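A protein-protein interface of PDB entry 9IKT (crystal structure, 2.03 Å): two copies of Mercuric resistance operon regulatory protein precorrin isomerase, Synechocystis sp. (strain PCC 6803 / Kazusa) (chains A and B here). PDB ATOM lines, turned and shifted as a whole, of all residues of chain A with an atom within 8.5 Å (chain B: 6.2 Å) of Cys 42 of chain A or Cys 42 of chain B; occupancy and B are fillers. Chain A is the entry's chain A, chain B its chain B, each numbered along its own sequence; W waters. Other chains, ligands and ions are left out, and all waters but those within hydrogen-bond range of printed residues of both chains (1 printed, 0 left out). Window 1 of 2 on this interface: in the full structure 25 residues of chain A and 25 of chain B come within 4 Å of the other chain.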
ATOM      1  N   LEU A  35     -18.061 -29.016  13.723  1.00  0.00           N
ATOM      2  CA  LEU A  35     -17.133 -29.563  14.703  1.00  0.00           C
ATOM      3  C   LEU A  35     -15.702 -29.601  14.150  1.00  0.00           C
ATOM      4  O   LEU A  35     -14.745 -29.306  14.876  1.00  0.00           O
ATOM      5  CB  LEU A  35     -17.597 -30.961  15.127  1.00  0.00           C
ATOM      6  CG  LEU A  35     -18.994 -31.100  15.739  1.00  0.00           C
ATOM      7  CD1 LEU A  35     -19.281 -32.561  16.048  1.00  0.00           C
ATOM      8  CD2 LEU A  35     -19.114 -30.271  17.000  1.00  0.00           C
ATOM      9  N   HIS A  36     -15.539 -29.937  12.869  1.00  0.00           N
ATOM     10  CA  HIS A  36     -14.217 -29.872  12.243  1.00  0.00           C
ATOM     11  C   HIS A  36     -13.645 -28.461  12.294  1.00  0.00           C
ATOM     12  O   HIS A  36     -12.457 -28.279  12.593  1.00  0.00           O
ATOM     13  CB  HIS A  36     -14.270 -30.338  10.789  1.00  0.00           C
ATOM     14  CG  HIS A  36     -14.352 -31.819  10.628  1.00  0.00           C
ATOM     15  ND1 HIS A  36     -13.865 -32.471   9.517  1.00  0.00           N
ATOM     16  CD2 HIS A  36     -14.871 -32.775  11.430  1.00  0.00           C
ATOM     17  CE1 HIS A  36     -14.080 -33.768   9.642  1.00  0.00           C
ATOM     18  NE2 HIS A  36     -14.689 -33.980  10.794  1.00  0.00           N
ATOM     19  N   GLN A  37     -14.472 -27.451  11.954  1.00  0.00           N
ATOM     20  CA  GLN A  37     -13.999 -26.067  11.960  1.00  0.00           C
ATOM     21  C   GLN A  37     -13.594 -25.644  13.359  1.00  0.00           C
ATOM     22  O   GLN A  37     -12.635 -24.886  13.532  1.00  0.00           O
ATOM     23  CB  GLN A  37     -15.067 -25.107  11.428  1.00  0.00           C
ATOM     24  CG  GLN A  37     -15.521 -25.378  10.024  1.00  0.00           C
ATOM     25  CD  GLN A  37     -14.370 -25.629   9.099  1.00  0.00           C
ATOM     26  OE1 GLN A  37     -13.550 -24.747   8.857  1.00  0.00           O
ATOM     27  NE2 GLN A  37     -14.248 -26.861   8.636  1.00  0.00           N
ATOM     28  N   LEU A  38     -14.310 -26.133  14.370  1.00  0.00           N
ATOM     29  CA  LEU A  38     -13.983 -25.776  15.744  1.00  0.00           C
ATOM     30  C   LEU A  38     -12.660 -26.398  16.175  1.00  0.00           C
ATOM     31  O   LEU A  38     -11.841 -25.734  16.818  1.00  0.00           O
ATOM     32  CB  LEU A  38     -15.121 -26.200  16.670  1.00  0.00           C
ATOM     33  CG  LEU A  38     -16.314 -25.234  16.648  1.00  0.00           C
ATOM     34  CD1 LEU A  38     -17.463 -25.805  17.446  1.00  0.00           C
ATOM     35  CD2 LEU A  38     -15.918 -23.865  17.189  1.00  0.00           C
ATOM     36  N   VAL A  39     -12.427 -27.664  15.818  1.00  0.00           N
ATOM     37  CA  VAL A  39     -11.140 -28.296  16.124  1.00  0.00           C
ATOM     38  C   VAL A  39     -10.010 -27.563  15.412  1.00  0.00           C
ATOM     39  O   VAL A  39      -8.964 -27.270  16.002  1.00  0.00           O
ATOM     40  CB  VAL A  39     -11.164 -29.790  15.748  1.00  0.00           C
ATOM     41  CG1 VAL A  39      -9.743 -30.376  15.789  1.00  0.00           C
ATOM     42  CG2 VAL A  39     -12.097 -30.561  16.679  1.00  0.00           C
ATOM     43  N   LEU A  40     -10.203 -27.269  14.126  1.00  0.00           N
ATOM     44  CA  LEU A  40      -9.231 -26.473  13.389  1.00  0.00           C
ATOM     45  C   LEU A  40      -8.982 -25.125  14.055  1.00  0.00           C
ATOM     46  O   LEU A  40      -7.881 -24.584  13.947  1.00  0.00           O
ATOM     47  CB  LEU A  40      -9.704 -26.259  11.952  1.00  0.00           C
ATOM     48  CG  LEU A  40      -9.700 -27.445  10.984  1.00  0.00           C
ATOM     49  CD1 LEU A  40     -10.336 -27.023   9.661  1.00  0.00           C
ATOM     50  CD2 LEU A  40      -8.307 -27.977  10.728  1.00  0.00           C
ATOM     51  N   ALA A  41      -9.979 -24.564  14.745  1.00  0.00           N
ATOM     52  CA  ALA A  41      -9.788 -23.245  15.343  1.00  0.00           C
ATOM     53  C   ALA A  41      -8.781 -23.288  16.486  1.00  0.00           C
ATOM     54  O   ALA A  41      -7.950 -22.382  16.624  1.00  0.00           O
ATOM     55  CB  ALA A  41     -11.122 -22.679  15.828  1.00  0.00           C
ATOM     56  N   CYS A  42      -8.820 -24.329  17.309  1.00  0.00           N
ATOM     57  CA  CYS A  42      -8.048 -24.306  18.540  1.00  0.00           C
ATOM     58  C   CYS A  42      -7.294 -25.594  18.822  1.00  0.00           C
ATOM     59  O   CYS A  42      -6.589 -25.659  19.835  1.00  0.00           O
ATOM     60  CB  CYS A  42      -8.957 -24.002  19.732  1.00  0.00           C
ATOM     61  SG  CYS A  42     -10.066 -25.358  20.067  1.00  0.00           S
ATOM     62  N   GLY A  43      -7.417 -26.612  17.968  1.00  0.00           N
ATOM     63  CA  GLY A  43      -6.655 -27.833  18.108  1.00  0.00           C
ATOM     64  C   GLY A  43      -7.179 -28.829  19.120  1.00  0.00           C
ATOM     65  O   GLY A  43      -6.618 -29.929  19.226  1.00  0.00           O
ATOM     66  N   ASP A  44      -8.226 -28.504  19.874  1.00  0.00           N
ATOM     67  CA  ASP A  44      -8.685 -29.396  20.938  1.00  0.00           C
ATOM     68  C   ASP A  44      -9.657 -30.410  20.348  1.00  0.00           C
ATOM     69  O   ASP A  44     -10.842 -30.123  20.165  1.00  0.00           O
ATOM     70  CB  ASP A  44      -9.306 -28.610  22.088  1.00  0.00           C
ATOM     71  CG  ASP A  44      -9.447 -29.447  23.362  1.00  0.00           C
ATOM     72  OD1 ASP A  44      -9.838 -30.631  23.260  1.00  0.00           O
ATOM     73  OD2 ASP A  44      -9.125 -28.941  24.459  1.00  0.00           O
ATOM     74  N   VAL A  45      -9.148 -31.614  20.076  1.00  0.00           N
ATOM     75  CA  VAL A  45      -9.951 -32.688  19.505  1.00  0.00           C
ATOM     76  C   VAL A  45     -11.126 -33.043  20.406  1.00  0.00           C
ATOM     77  O   VAL A  45     -12.155 -33.543  19.935  1.00  0.00           O
ATOM     78  CB  VAL A  45      -9.046 -33.905  19.235  1.00  0.00           C
ATOM     79  CG1 VAL A  45      -9.870 -35.108  18.844  1.00  0.00           C
ATOM     80  CG2 VAL A  45      -8.040 -33.577  18.145  1.00  0.00           C
ATOM     81  N   SER A  46     -11.007 -32.788  21.708  1.00  0.00           N
ATOM     82  CA  SER A  46     -12.087 -33.139  22.618  1.00  0.00           C
ATOM     83  C   SER A  46     -13.326 -32.275  22.418  1.00  0.00           C
ATOM     84  O   SER A  46     -14.385 -32.614  22.957  1.00  0.00           O
ATOM     85  CB  SER A  46     -11.609 -33.029  24.071  1.00  0.00           C
ATOM     86  OG  SER A  46     -11.789 -31.699  24.545  1.00  0.00           O
ATOM     87  N   LEU A  47     -13.225 -31.179  21.654  1.00  0.00           N
ATOM     88  CA  LEU A  47     -14.398 -30.357  21.382  1.00  0.00           C
ATOM     89  C   LEU A  47     -15.505 -31.156  20.715  1.00  0.00           C
ATOM     90  O   LEU A  47     -16.684 -30.825  20.884  1.00  0.00           O
ATOM     91  CB  LEU A  47     -14.036 -29.160  20.500  1.00  0.00           C
ATOM     92  CG  LEU A  47     -13.710 -27.840  21.192  1.00  0.00           C
ATOM     93  CD1 LEU A  47     -13.296 -26.810  20.156  1.00  0.00           C
ATOM     94  CD2 LEU A  47     -14.911 -27.340  21.999  1.00  0.00           C
ATOM     95  N   GLY A 135     -19.119 -14.768  23.173  1.00  0.00           N
ATOM     96  CA  GLY A 135     -17.809 -15.385  23.252  1.00  0.00           C
ATOM     97  C   GLY A 135     -16.966 -14.969  24.439  1.00  0.00           C
ATOM     98  O   GLY A 135     -15.810 -15.380  24.540  1.00  0.00           O
ATOM     99  N   MET A 161     -20.890 -19.193  24.307  1.00  0.00           N
ATOM    100  CA  MET A 161     -19.520 -19.697  24.443  1.00  0.00           C
ATOM    101  C   MET A 161     -18.635 -18.750  25.251  1.00  0.00           C
ATOM    102  O   MET A 161     -17.529 -18.410  24.829  1.00  0.00           O
ATOM    103  CB  MET A 161     -18.954 -19.926  23.050  1.00  0.00           C
ATOM    104  CG  MET A 161     -19.338 -21.281  22.522  1.00  0.00           C
ATOM    105  SD  MET A 161     -18.939 -21.572  20.799  1.00  0.00           S
ATOM    106  CE  MET A 161     -20.130 -22.860  20.398  1.00  0.00           C
ATOM    107  N   PRO A 162     -19.089 -18.315  26.438  1.00  0.00           N
ATOM    108  CA  PRO A 162     -18.258 -17.424  27.259  1.00  0.00           C
ATOM    109  C   PRO A 162     -16.974 -18.102  27.713  1.00  0.00           C
ATOM    110  O   PRO A 162     -16.859 -19.331  27.736  1.00  0.00           O
ATOM    111  CB  PRO A 162     -19.151 -17.122  28.468  1.00  0.00           C
ATOM    112  CG  PRO A 162     -19.975 -18.360  28.607  1.00  0.00           C
ATOM    113  CD  PRO A 162     -20.283 -18.769  27.183  1.00  0.00           C
ATOM    114  N   ILE A 163     -16.014 -17.262  28.115  1.00  0.00           N
ATOM    115  CA  ILE A 163     -14.807 -17.739  28.784  1.00  0.00           C
ATOM    116  C   ILE A 163     -15.187 -18.371  30.127  1.00  0.00           C
ATOM    117  O   ILE A 163     -16.227 -18.048  30.718  1.00  0.00           O
ATOM    118  CB  ILE A 163     -13.827 -16.563  28.962  1.00  0.00           C
ATOM    119  CG1 ILE A 163     -13.424 -16.037  27.593  1.00  0.00           C
ATOM    120  CG2 ILE A 163     -12.581 -16.948  29.707  1.00  0.00           C
ATOM    121  CD1 ILE A 163     -12.855 -17.114  26.758  1.00  0.00           C
ATOM    122  N   GLY A 164     -14.330 -19.274  30.613  1.00  0.00           N
ATOM    123  CA  GLY A 164     -14.581 -20.037  31.822  1.00  0.00           C
ATOM    124  C   GLY A 164     -14.430 -19.296  33.137  1.00  0.00           C
ATOM    125  O   GLY A 164     -13.845 -19.832  34.083  1.00  0.00           O
ATOM    126  N   ILE A 185     -20.973 -25.115  24.777  1.00  0.00           N
ATOM    127  CA  ILE A 185     -19.876 -26.047  25.042  1.00  0.00           C
ATOM    128  C   ILE A 185     -19.939 -26.499  26.491  1.00  0.00           C
ATOM    129  O   ILE A 185     -19.875 -25.675  27.410  1.00  0.00           O
ATOM    130  CB  ILE A 185     -18.499 -25.438  24.748  1.00  0.00           C
ATOM    131  CG1 ILE A 185     -18.377 -25.095  23.269  1.00  0.00           C
ATOM    132  CG2 ILE A 185     -17.391 -26.426  25.167  1.00  0.00           C
ATOM    133  CD1 ILE A 185     -17.230 -24.191  22.957  1.00  0.00           C
ATOM    134  N   SER A 188     -14.792 -26.127  29.806  1.00  0.00           N
ATOM    135  CA  SER A 188     -14.150 -24.839  30.035  1.00  0.00           C
ATOM    136  C   SER A 188     -13.888 -24.044  28.761  1.00  0.00           C
ATOM    137  O   SER A 188     -13.810 -22.814  28.833  1.00  0.00           O
ATOM    138  CB  SER A 188     -12.829 -25.030  30.794  1.00  0.00           C
ATOM    139  OG  SER A 188     -11.765 -25.279  29.894  1.00  0.00           O
ATOM    140  N   LEU A 189     -13.761 -24.700  27.607  1.00  0.00           N
ATOM    141  CA  LEU A 189     -13.495 -23.999  26.355  1.00  0.00           C
ATOM    142  C   LEU A 189     -14.619 -23.017  25.999  1.00  0.00           C
ATOM    143  O   LEU A 189     -15.754 -23.137  26.452  1.00  0.00           O
ATOM    144  CB  LEU A 189     -13.319 -24.992  25.215  1.00  0.00           C
ATOM    145  CG  LEU A 189     -12.245 -26.049  25.451  1.00  0.00           C
ATOM    146  CD1 LEU A 189     -11.917 -26.756  24.154  1.00  0.00           C
ATOM    147  CD2 LEU A 189     -10.995 -25.398  26.029  1.00  0.00           C
ATOM    148  N   GLY A 190     -14.278 -22.067  25.134  1.00  0.00           N
ATOM    149  CA  GLY A 190     -15.143 -20.961  24.771  1.00  0.00           C
ATOM    150  C   GLY A 190     -14.291 -19.899  24.099  1.00  0.00           C
ATOM    151  O   GLY A 190     -13.124 -20.134  23.823  1.00  0.00           O
ATOM    152  N   GLY A 191     -14.862 -18.733  23.852  1.00  0.00           N
ATOM    153  CA  GLY A 191     -14.041 -17.595  23.491  1.00  0.00           C
ATOM    154  C   GLY A 191     -14.490 -16.927  22.211  1.00  0.00           C
ATOM    155  O   GLY A 191     -15.413 -17.370  21.521  1.00  0.00           O
ATOM    156  N   GLY A 192     -13.821 -15.816  21.912  1.00  0.00           N
ATOM    157  CA  GLY A 192     -14.253 -14.988  20.802  1.00  0.00           C
ATOM    158  C   GLY A 192     -14.134 -15.721  19.485  1.00  0.00           C
ATOM    159  O   GLY A 192     -15.063 -15.723  18.666  1.00  0.00           O
ATOM    160  N   LEU A 193     -12.998 -16.383  19.277  1.00  0.00           N
ATOM    161  CA  LEU A 193     -12.827 -17.139  18.052  1.00  0.00           C
ATOM    162  C   LEU A 193     -13.847 -18.261  17.973  1.00  0.00           C
ATOM    163  O   LEU A 193     -14.467 -18.468  16.922  1.00  0.00           O
ATOM    164  CB  LEU A 193     -11.402 -17.687  17.973  1.00  0.00           C
ATOM    165  CG  LEU A 193     -10.926 -18.337  16.670  1.00  0.00           C
ATOM    166  CD1 LEU A 193     -11.133 -17.382  15.492  1.00  0.00           C
ATOM    167  CD2 LEU A 193      -9.461 -18.726  16.796  1.00  0.00           C
ATOM    168  N   LEU A 194     -14.047 -18.996  19.075  1.00  0.00           N
ATOM    169  CA  LEU A 194     -14.897 -20.178  18.983  1.00  0.00           C
ATOM    170  C   LEU A 194     -16.323 -19.793  18.636  1.00  0.00           C
ATOM    171  O   LEU A 194     -16.962 -20.456  17.807  1.00  0.00           O
ATOM    172  CB  LEU A 194     -14.858 -20.986  20.280  1.00  0.00           C
ATOM    173  CG  LEU A 194     -13.537 -21.723  20.601  1.00  0.00           C
ATOM    174  CD1 LEU A 194     -13.825 -22.825  21.594  1.00  0.00           C
ATOM    175  CD2 LEU A 194     -12.830 -22.292  19.381  1.00  0.00           C
ATOM    176  N   ALA A 195     -16.842 -18.724  19.258  1.00  0.00           N
ATOM    177  CA  ALA A 195     -18.197 -18.278  18.931  1.00  0.00           C
ATOM    178  C   ALA A 195     -18.279 -17.804  17.487  1.00  0.00           C
ATOM    179  O   ALA A 195     -19.227 -18.132  16.776  1.00  0.00           O
ATOM    180  CB  ALA A 195     -18.646 -17.169  19.891  1.00  0.00           C
ATOM    181  N   VAL A 197     -16.209 -18.652  14.950  1.00  0.00           N
ATOM    182  CA  VAL A 197     -15.996 -19.776  14.045  1.00  0.00           C
ATOM    183  C   VAL A 197     -17.285 -20.568  13.879  1.00  0.00           C
ATOM    184  O   VAL A 197     -17.599 -21.056  12.782  1.00  0.00           O
ATOM    185  CB  VAL A 197     -14.835 -20.655  14.555  1.00  0.00           C
ATOM    186  CG1 VAL A 197     -14.859 -22.020  13.888  1.00  0.00           C
ATOM    187  CG2 VAL A 197     -13.498 -19.961  14.279  1.00  0.00           C
ATOM    188  N   GLN B  37      -4.630 -12.671  24.210  1.00  0.00           N
ATOM    189  CA  GLN B  37      -5.351 -12.911  22.960  1.00  0.00           C
ATOM    190  C   GLN B  37      -5.595 -14.397  22.742  1.00  0.00           C
ATOM    191  O   GLN B  37      -6.693 -14.802  22.339  1.00  0.00           O
ATOM    192  CB  GLN B  37      -4.593 -12.309  21.773  1.00  0.00           C
ATOM    193  CG  GLN B  37      -4.550 -10.786  21.765  1.00  0.00           C
ATOM    194  CD  GLN B  37      -5.945 -10.165  21.736  1.00  0.00           C
ATOM    195  OE1 GLN B  37      -6.501  -9.856  22.766  1.00  0.00           O
ATOM    196  NE2 GLN B  37      -6.507  -9.996  20.546  1.00  0.00           N
ATOM    197  N   LEU B  38      -4.591 -15.228  23.028  1.00  0.00           N
ATOM    198  CA  LEU B  38      -4.759 -16.670  22.879  1.00  0.00           C
ATOM    199  C   LEU B  38      -5.846 -17.212  23.804  1.00  0.00           C
ATOM    200  O   LEU B  38      -6.675 -18.032  23.385  1.00  0.00           O
ATOM    201  CB  LEU B  38      -3.426 -17.362  23.138  1.00  0.00           C
ATOM    202  CG  LEU B  38      -2.336 -16.982  22.138  1.00  0.00           C
ATOM    203  CD1 LEU B  38      -0.971 -17.530  22.567  1.00  0.00           C
ATOM    204  CD2 LEU B  38      -2.699 -17.499  20.755  1.00  0.00           C
ATOM    205  N   VAL B  39      -5.867 -16.762  25.063  1.00  0.00           N
ATOM    206  CA  VAL B  39      -6.887 -17.223  26.005  1.00  0.00           C
ATOM    207  C   VAL B  39      -8.266 -16.703  25.610  1.00  0.00           C
ATOM    208  O   VAL B  39      -9.270 -17.425  25.706  1.00  0.00           O
ATOM    209  CB  VAL B  39      -6.508 -16.808  27.440  1.00  0.00           C
ATOM    210  CG1 VAL B  39      -7.677 -17.014  28.402  1.00  0.00           C
ATOM    211  CG2 VAL B  39      -5.261 -17.595  27.909  1.00  0.00           C
ATOM    212  N   LEU B  40      -8.345 -15.446  25.166  1.00  0.00           N
ATOM    213  CA  LEU B  40      -9.627 -14.917  24.708  1.00  0.00           C
ATOM    214  C   LEU B  40     -10.156 -15.689  23.510  1.00  0.00           C
ATOM    215  O   LEU B  40     -11.376 -15.786  23.328  1.00  0.00           O
ATOM    216  CB  LEU B  40      -9.487 -13.445  24.340  1.00  0.00           C
ATOM    217  CG  LEU B  40      -9.409 -12.495  25.521  1.00  0.00           C
ATOM    218  CD1 LEU B  40      -9.059 -11.084  25.053  1.00  0.00           C
ATOM    219  CD2 LEU B  40     -10.730 -12.529  26.242  1.00  0.00           C
ATOM    220  N   ALA B  41      -9.259 -16.232  22.679  1.00  0.00           N
ATOM    221  CA  ALA B  41      -9.689 -16.872  21.440  1.00  0.00           C
ATOM    222  C   ALA B  41     -10.308 -18.239  21.691  1.00  0.00           C
ATOM    223  O   ALA B  41     -11.319 -18.588  21.068  1.00  0.00           O
ATOM    224  CB  ALA B  41      -8.515 -17.003  20.467  1.00  0.00           C
ATOM    225  N   CYS B  42      -9.730 -19.026  22.601  1.00  0.00           N
ATOM    226  CA  CYS B  42     -10.161 -20.404  22.774  1.00  0.00           C
ATOM    227  C   CYS B  42     -10.468 -20.797  24.209  1.00  0.00           C
ATOM    228  O   CYS B  42     -10.985 -21.899  24.421  1.00  0.00           O
ATOM    229  CB  CYS B  42      -9.101 -21.359  22.225  1.00  0.00           C
ATOM    230  SG  CYS B  42      -7.640 -21.432  23.308  1.00  0.00           S
ATOM    231  N   GLY B  43     -10.171 -19.954  25.194  1.00  0.00           N
ATOM    232  CA  GLY B  43     -10.606 -20.203  26.555  1.00  0.00           C
ATOM    233  C   GLY B  43      -9.674 -21.039  27.411  1.00  0.00           C
ATOM    234  O   GLY B  43      -9.946 -21.215  28.607  1.00  0.00           O
ATOM    235  N   ASP B  44      -8.576 -21.544  26.857  1.00  0.00           N
ATOM    236  CA  ASP B  44      -7.697 -22.454  27.591  1.00  0.00           C
ATOM    237  C   ASP B  44      -6.708 -21.634  28.406  1.00  0.00           C
ATOM    238  O   ASP B  44      -5.687 -21.168  27.886  1.00  0.00           O
ATOM    239  CB  ASP B  44      -6.977 -23.393  26.626  1.00  0.00           C
ATOM    240  CG  ASP B  44      -6.066 -24.375  27.344  1.00  0.00           C
ATOM    241  OD1 ASP B  44      -6.179 -24.476  28.588  1.00  0.00           O
ATOM    242  OD2 ASP B  44      -5.240 -25.042  26.668  1.00  0.00           O
ATOM    243  N   LEU B  47      -2.783 -22.151  28.417  1.00  0.00           N
ATOM    244  CA  LEU B  47      -1.874 -21.604  27.419  1.00  0.00           C
ATOM    245  C   LEU B  47      -0.848 -20.663  28.042  1.00  0.00           C
ATOM    246  O   LEU B  47       0.250 -20.496  27.497  1.00  0.00           O
ATOM    247  CB  LEU B  47      -2.676 -20.887  26.329  1.00  0.00           C
ATOM    248  CG  LEU B  47      -3.421 -21.785  25.338  1.00  0.00           C
ATOM    249  CD1 LEU B  47      -4.311 -20.958  24.411  1.00  0.00           C
ATOM    250  CD2 LEU B  47      -2.439 -22.591  24.536  1.00  0.00           C
ATOM    251  N   ILE B 163      -1.874 -28.842  14.091  1.00  0.00           N
ATOM    252  CA  ILE B 163      -2.883 -29.699  14.708  1.00  0.00           C
ATOM    253  C   ILE B 163      -2.231 -31.008  15.174  1.00  0.00           C
ATOM    254  O   ILE B 163      -1.258 -31.483  14.582  1.00  0.00           O
ATOM    255  CB  ILE B 163      -4.010 -29.957  13.689  1.00  0.00           C
ATOM    256  CG1 ILE B 163      -4.812 -28.668  13.431  1.00  0.00           C
ATOM    257  CG2 ILE B 163      -4.916 -31.100  14.117  1.00  0.00           C
ATOM    258  CD1 ILE B 163      -5.456 -28.099  14.668  1.00  0.00           C
ATOM    259  N   LEU B 189      -3.184 -28.965  23.940  1.00  0.00           N
ATOM    260  CA  LEU B 189      -3.661 -29.384  22.629  1.00  0.00           C
ATOM    261  C   LEU B 189      -3.828 -28.217  21.663  1.00  0.00           C
ATOM    262  O   LEU B 189      -4.321 -28.419  20.552  1.00  0.00           O
ATOM    263  CB  LEU B 189      -4.990 -30.137  22.766  1.00  0.00           C
ATOM    264  N   GLY B 190      -3.420 -27.010  22.056  1.00  0.00           N
ATOM    265  CA  GLY B 190      -3.627 -25.854  21.203  1.00  0.00           C
ATOM    266  C   GLY B 190      -2.892 -25.977  19.876  1.00  0.00           C
ATOM    267  O   GLY B 190      -1.789 -26.515  19.795  1.00  0.00           O
ATOM    268  N   GLY B 191      -3.526 -25.447  18.834  1.00  0.00           N
ATOM    269  CA  GLY B 191      -2.935 -25.375  17.512  1.00  0.00           C
ATOM    270  C   GLY B 191      -3.976 -24.794  16.586  1.00  0.00           C
ATOM    271  O   GLY B 191      -4.964 -24.223  17.052  1.00  0.00           O
ATOM    272  N   GLY B 192      -3.773 -24.938  15.277  1.00  0.00           N
ATOM    273  CA  GLY B 192      -4.801 -24.469  14.345  1.00  0.00           C
ATOM    274  C   GLY B 192      -4.738 -22.966  14.153  1.00  0.00           C
ATOM    275  O   GLY B 192      -3.656 -22.384  14.032  1.00  0.00           O
ATOM    276  N   LEU B 193      -5.917 -22.319  14.159  1.00  0.00           N
ATOM    277  CA  LEU B 193      -6.033 -20.872  13.962  1.00  0.00           C
ATOM    278  C   LEU B 193      -5.410 -20.066  15.094  1.00  0.00           C
ATOM    279  O   LEU B 193      -5.326 -18.839  14.989  1.00  0.00           O
ATOM    280  CB  LEU B 193      -7.504 -20.454  13.808  1.00  0.00           C
ATOM    281  CG  LEU B 193      -8.281 -21.054  12.624  1.00  0.00           C
ATOM    282  CD1 LEU B 193      -9.592 -20.293  12.339  1.00  0.00           C
ATOM    283  CD2 LEU B 193      -7.399 -21.087  11.383  1.00  0.00           C
ATOM    284  N   LEU B 194      -4.999 -20.712  16.181  1.00  0.00           N
ATOM    285  CA  LEU B 194      -4.197 -20.018  17.175  1.00  0.00           C
ATOM    286  C   LEU B 194      -2.897 -19.504  16.578  1.00  0.00           C
ATOM    287  O   LEU B 194      -2.304 -18.562  17.112  1.00  0.00           O
ATOM    288  CB  LEU B 194      -3.904 -20.951  18.349  1.00  0.00           C
ATOM    289  CG  LEU B 194      -5.121 -21.477  19.117  1.00  0.00           C
ATOM    290  CD1 LEU B 194      -4.653 -22.309  20.304  1.00  0.00           C
ATOM    291  CD2 LEU B 194      -5.988 -20.337  19.581  1.00  0.00           C
HETATM  292  O   HOH W   1     -12.272 -20.941  29.781  1.00  0.00           O
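O of Leu 40 of chain A lies within hydrogen-bond range of N of Leu 193 of chain B (3.0 Å).
O of Ala 41 of chain A sits at hydrogen-bond distance from N of Leu 193 of chain B.
The backbone carbonyl oxygen (O) of Ala 41 of chain A lies within hydrogen-bond range of the backbone NH (N) of Leu 194 of chain B (3.4 Å).
O of Cys 42 of chain A lies within hydrogen-bond range of N of Gly 191 of chain B.
The backbone NH of Gly 190 of chain A sits at hydrogen-bond distance from the backbone carbonyl oxygen of Cys 42 of chain B.
The backbone carbonyl oxygen (O) of Gly 190 of chain A lies within hydrogen-bond range of the backbone NH (N) of Gly 43 of chain B (3.3 Å).
N of Gly 192 of chain A lies within hydrogen-bond range of O of Leu 40 of chain B, at 2.8 Å.
The backbone NH (N) of Leu 193 of chain A sits close to the backbone carbonyl oxygen (O) of Ala 41 of chain B, at 3.3 Å.
The backbone carbonyl oxygen of Ala 41 of chain B is in hydrogen-bond range of the backbone NH of Leu 194 of chain A.
O of Leu 189 of chain B lies close to O of Gly 43 of chain A, 3.1 Å away.
The backbone carbonyl oxygen (O) of Leu 38 of chain A lies within hydrogen-bond range of the side-chain sulfur (SG) of Cys 42 of chain A (3.7 Å).
N of Asp 44 of chain A sits close to SG of Cys 42 of chain A.
The side-chain sulfur (SG) of Cys 42 of chain B sits close to the backbone NH (N) of Asp 44 of chain B (3.7 Å).
Among the printed residues, pairs that only touch across the chains: Leu 40 of chain A with Gly 192 of chain B, Gly 191 of chain A with Leu 40 of chain B, Cys 42 of chain A with Gly 190 of chain B, Ala 41 of chain A with Gly 191 of chain B, Gly 43 of chain A with Gly 191 of chain B, Cys 42 of chain A with Cys 42 of chain B, Gly 190 of chain A with Ala 41 of chain B, Cys 42 of chain A with Leu 189 of chain B, Gly 43 of chain A with Ile 163 of chain B, Ile 163 of chain A with Val 39 of chain B, Gly 191 of chain A with Ala 41 of chain B, Leu 189 of chain A with Cys 42 of chain B, Ile 163 of chain A with Gly 43 of chain B, Gly 192 of chain A with Ala 41 of chain B, Val 39 of chain A with Ile 163 of chain B, Cys 42 of chain A with Leu 194 of chain B, Ile 163 of chain A with Leu 40 of chain B, Asp 44 of chain A with Leu 189 of chain B and Leu 193 of chain A with Leu 193 of chain B.
Gln 37 of chain A touches none of the printed residues of chain B.
Of the printed residues of chain B, Gly 43 of chain A touches Ile 163 (3.7 Å), Leu 189 (3.1 Å) and Gly 191 (3.5 Å).
Of the printed residues of chain B, Gly 190 of chain A touches Ala 41, Cys 42 and Gly 43.
Of chain A, only Gly 190 (3.6 Å), Gly 191 (3.8 Å), Gly 192 (3.8 Å), Leu 193 (3.2 Å) and Leu 194 (3.4 Å) come within 4 Å of Ala 41 of chain B.
Cys 42 of chain B touches just these residues of chain A: Cys 42, Leu 189 and Gly 190.
Of chain A, only Ile 163 and Gly 190 come within 4 Å of Gly 43 of chain B.
Of chain A, only Ala 41 (3.5 Å), Cys 42 (3.2 Å) and Gly 43 (3.5 Å) come within 4 Å of Gly 191 of chain B.
The nearest residue of chain A that does not touch Cys 42 of chain B is Leu 194 of chain A (4.1 Å).
The nearest printed residue of chain A that does not touch Ile 163 of chain B is Leu 40 of chain A (4.3 Å).
Of the 16 printed residues of chain B, 12 touch a printed residue of chain A.
Of the 28 printed residues of chain A, 13 touch a printed residue of chain B.
Printed residues of chain A that touch a printed residue of chain B: Val 39, Leu 40, Ala 41, Cys 42, Gly 43, Asp 44, Ile 163, Leu 189, Gly 190, Gly 191, Gly 192, Leu 193 and Leu 194.
Along chain A the printed residues that touch a printed residue of chain B span positions 39 to 194.
Ala 41 of chain A touches Gly 191 of chain B, and with the chains exchanged Gly 191 of chain A touches Ala 41 of chain B.
Cys 42 of chain A touches Gly 190 of chain B, and with the chains exchanged Gly 190 of chain A touches Cys 42 of chain B.
Of the 29 pairs that touch across the chains among the printed residues, 18 have their exchanged pair printed and touching as well.
Water W1 lies within hydrogen-bond range of the backbone carbonyl oxygen (O) of Ser 188 of chain A (2.6 Å), the backbone carbonyl oxygen (O) of Gly 43 of chain B (2.6 Å) and the backbone NH (N) of Gly 164 of chain A (2.8 Å).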
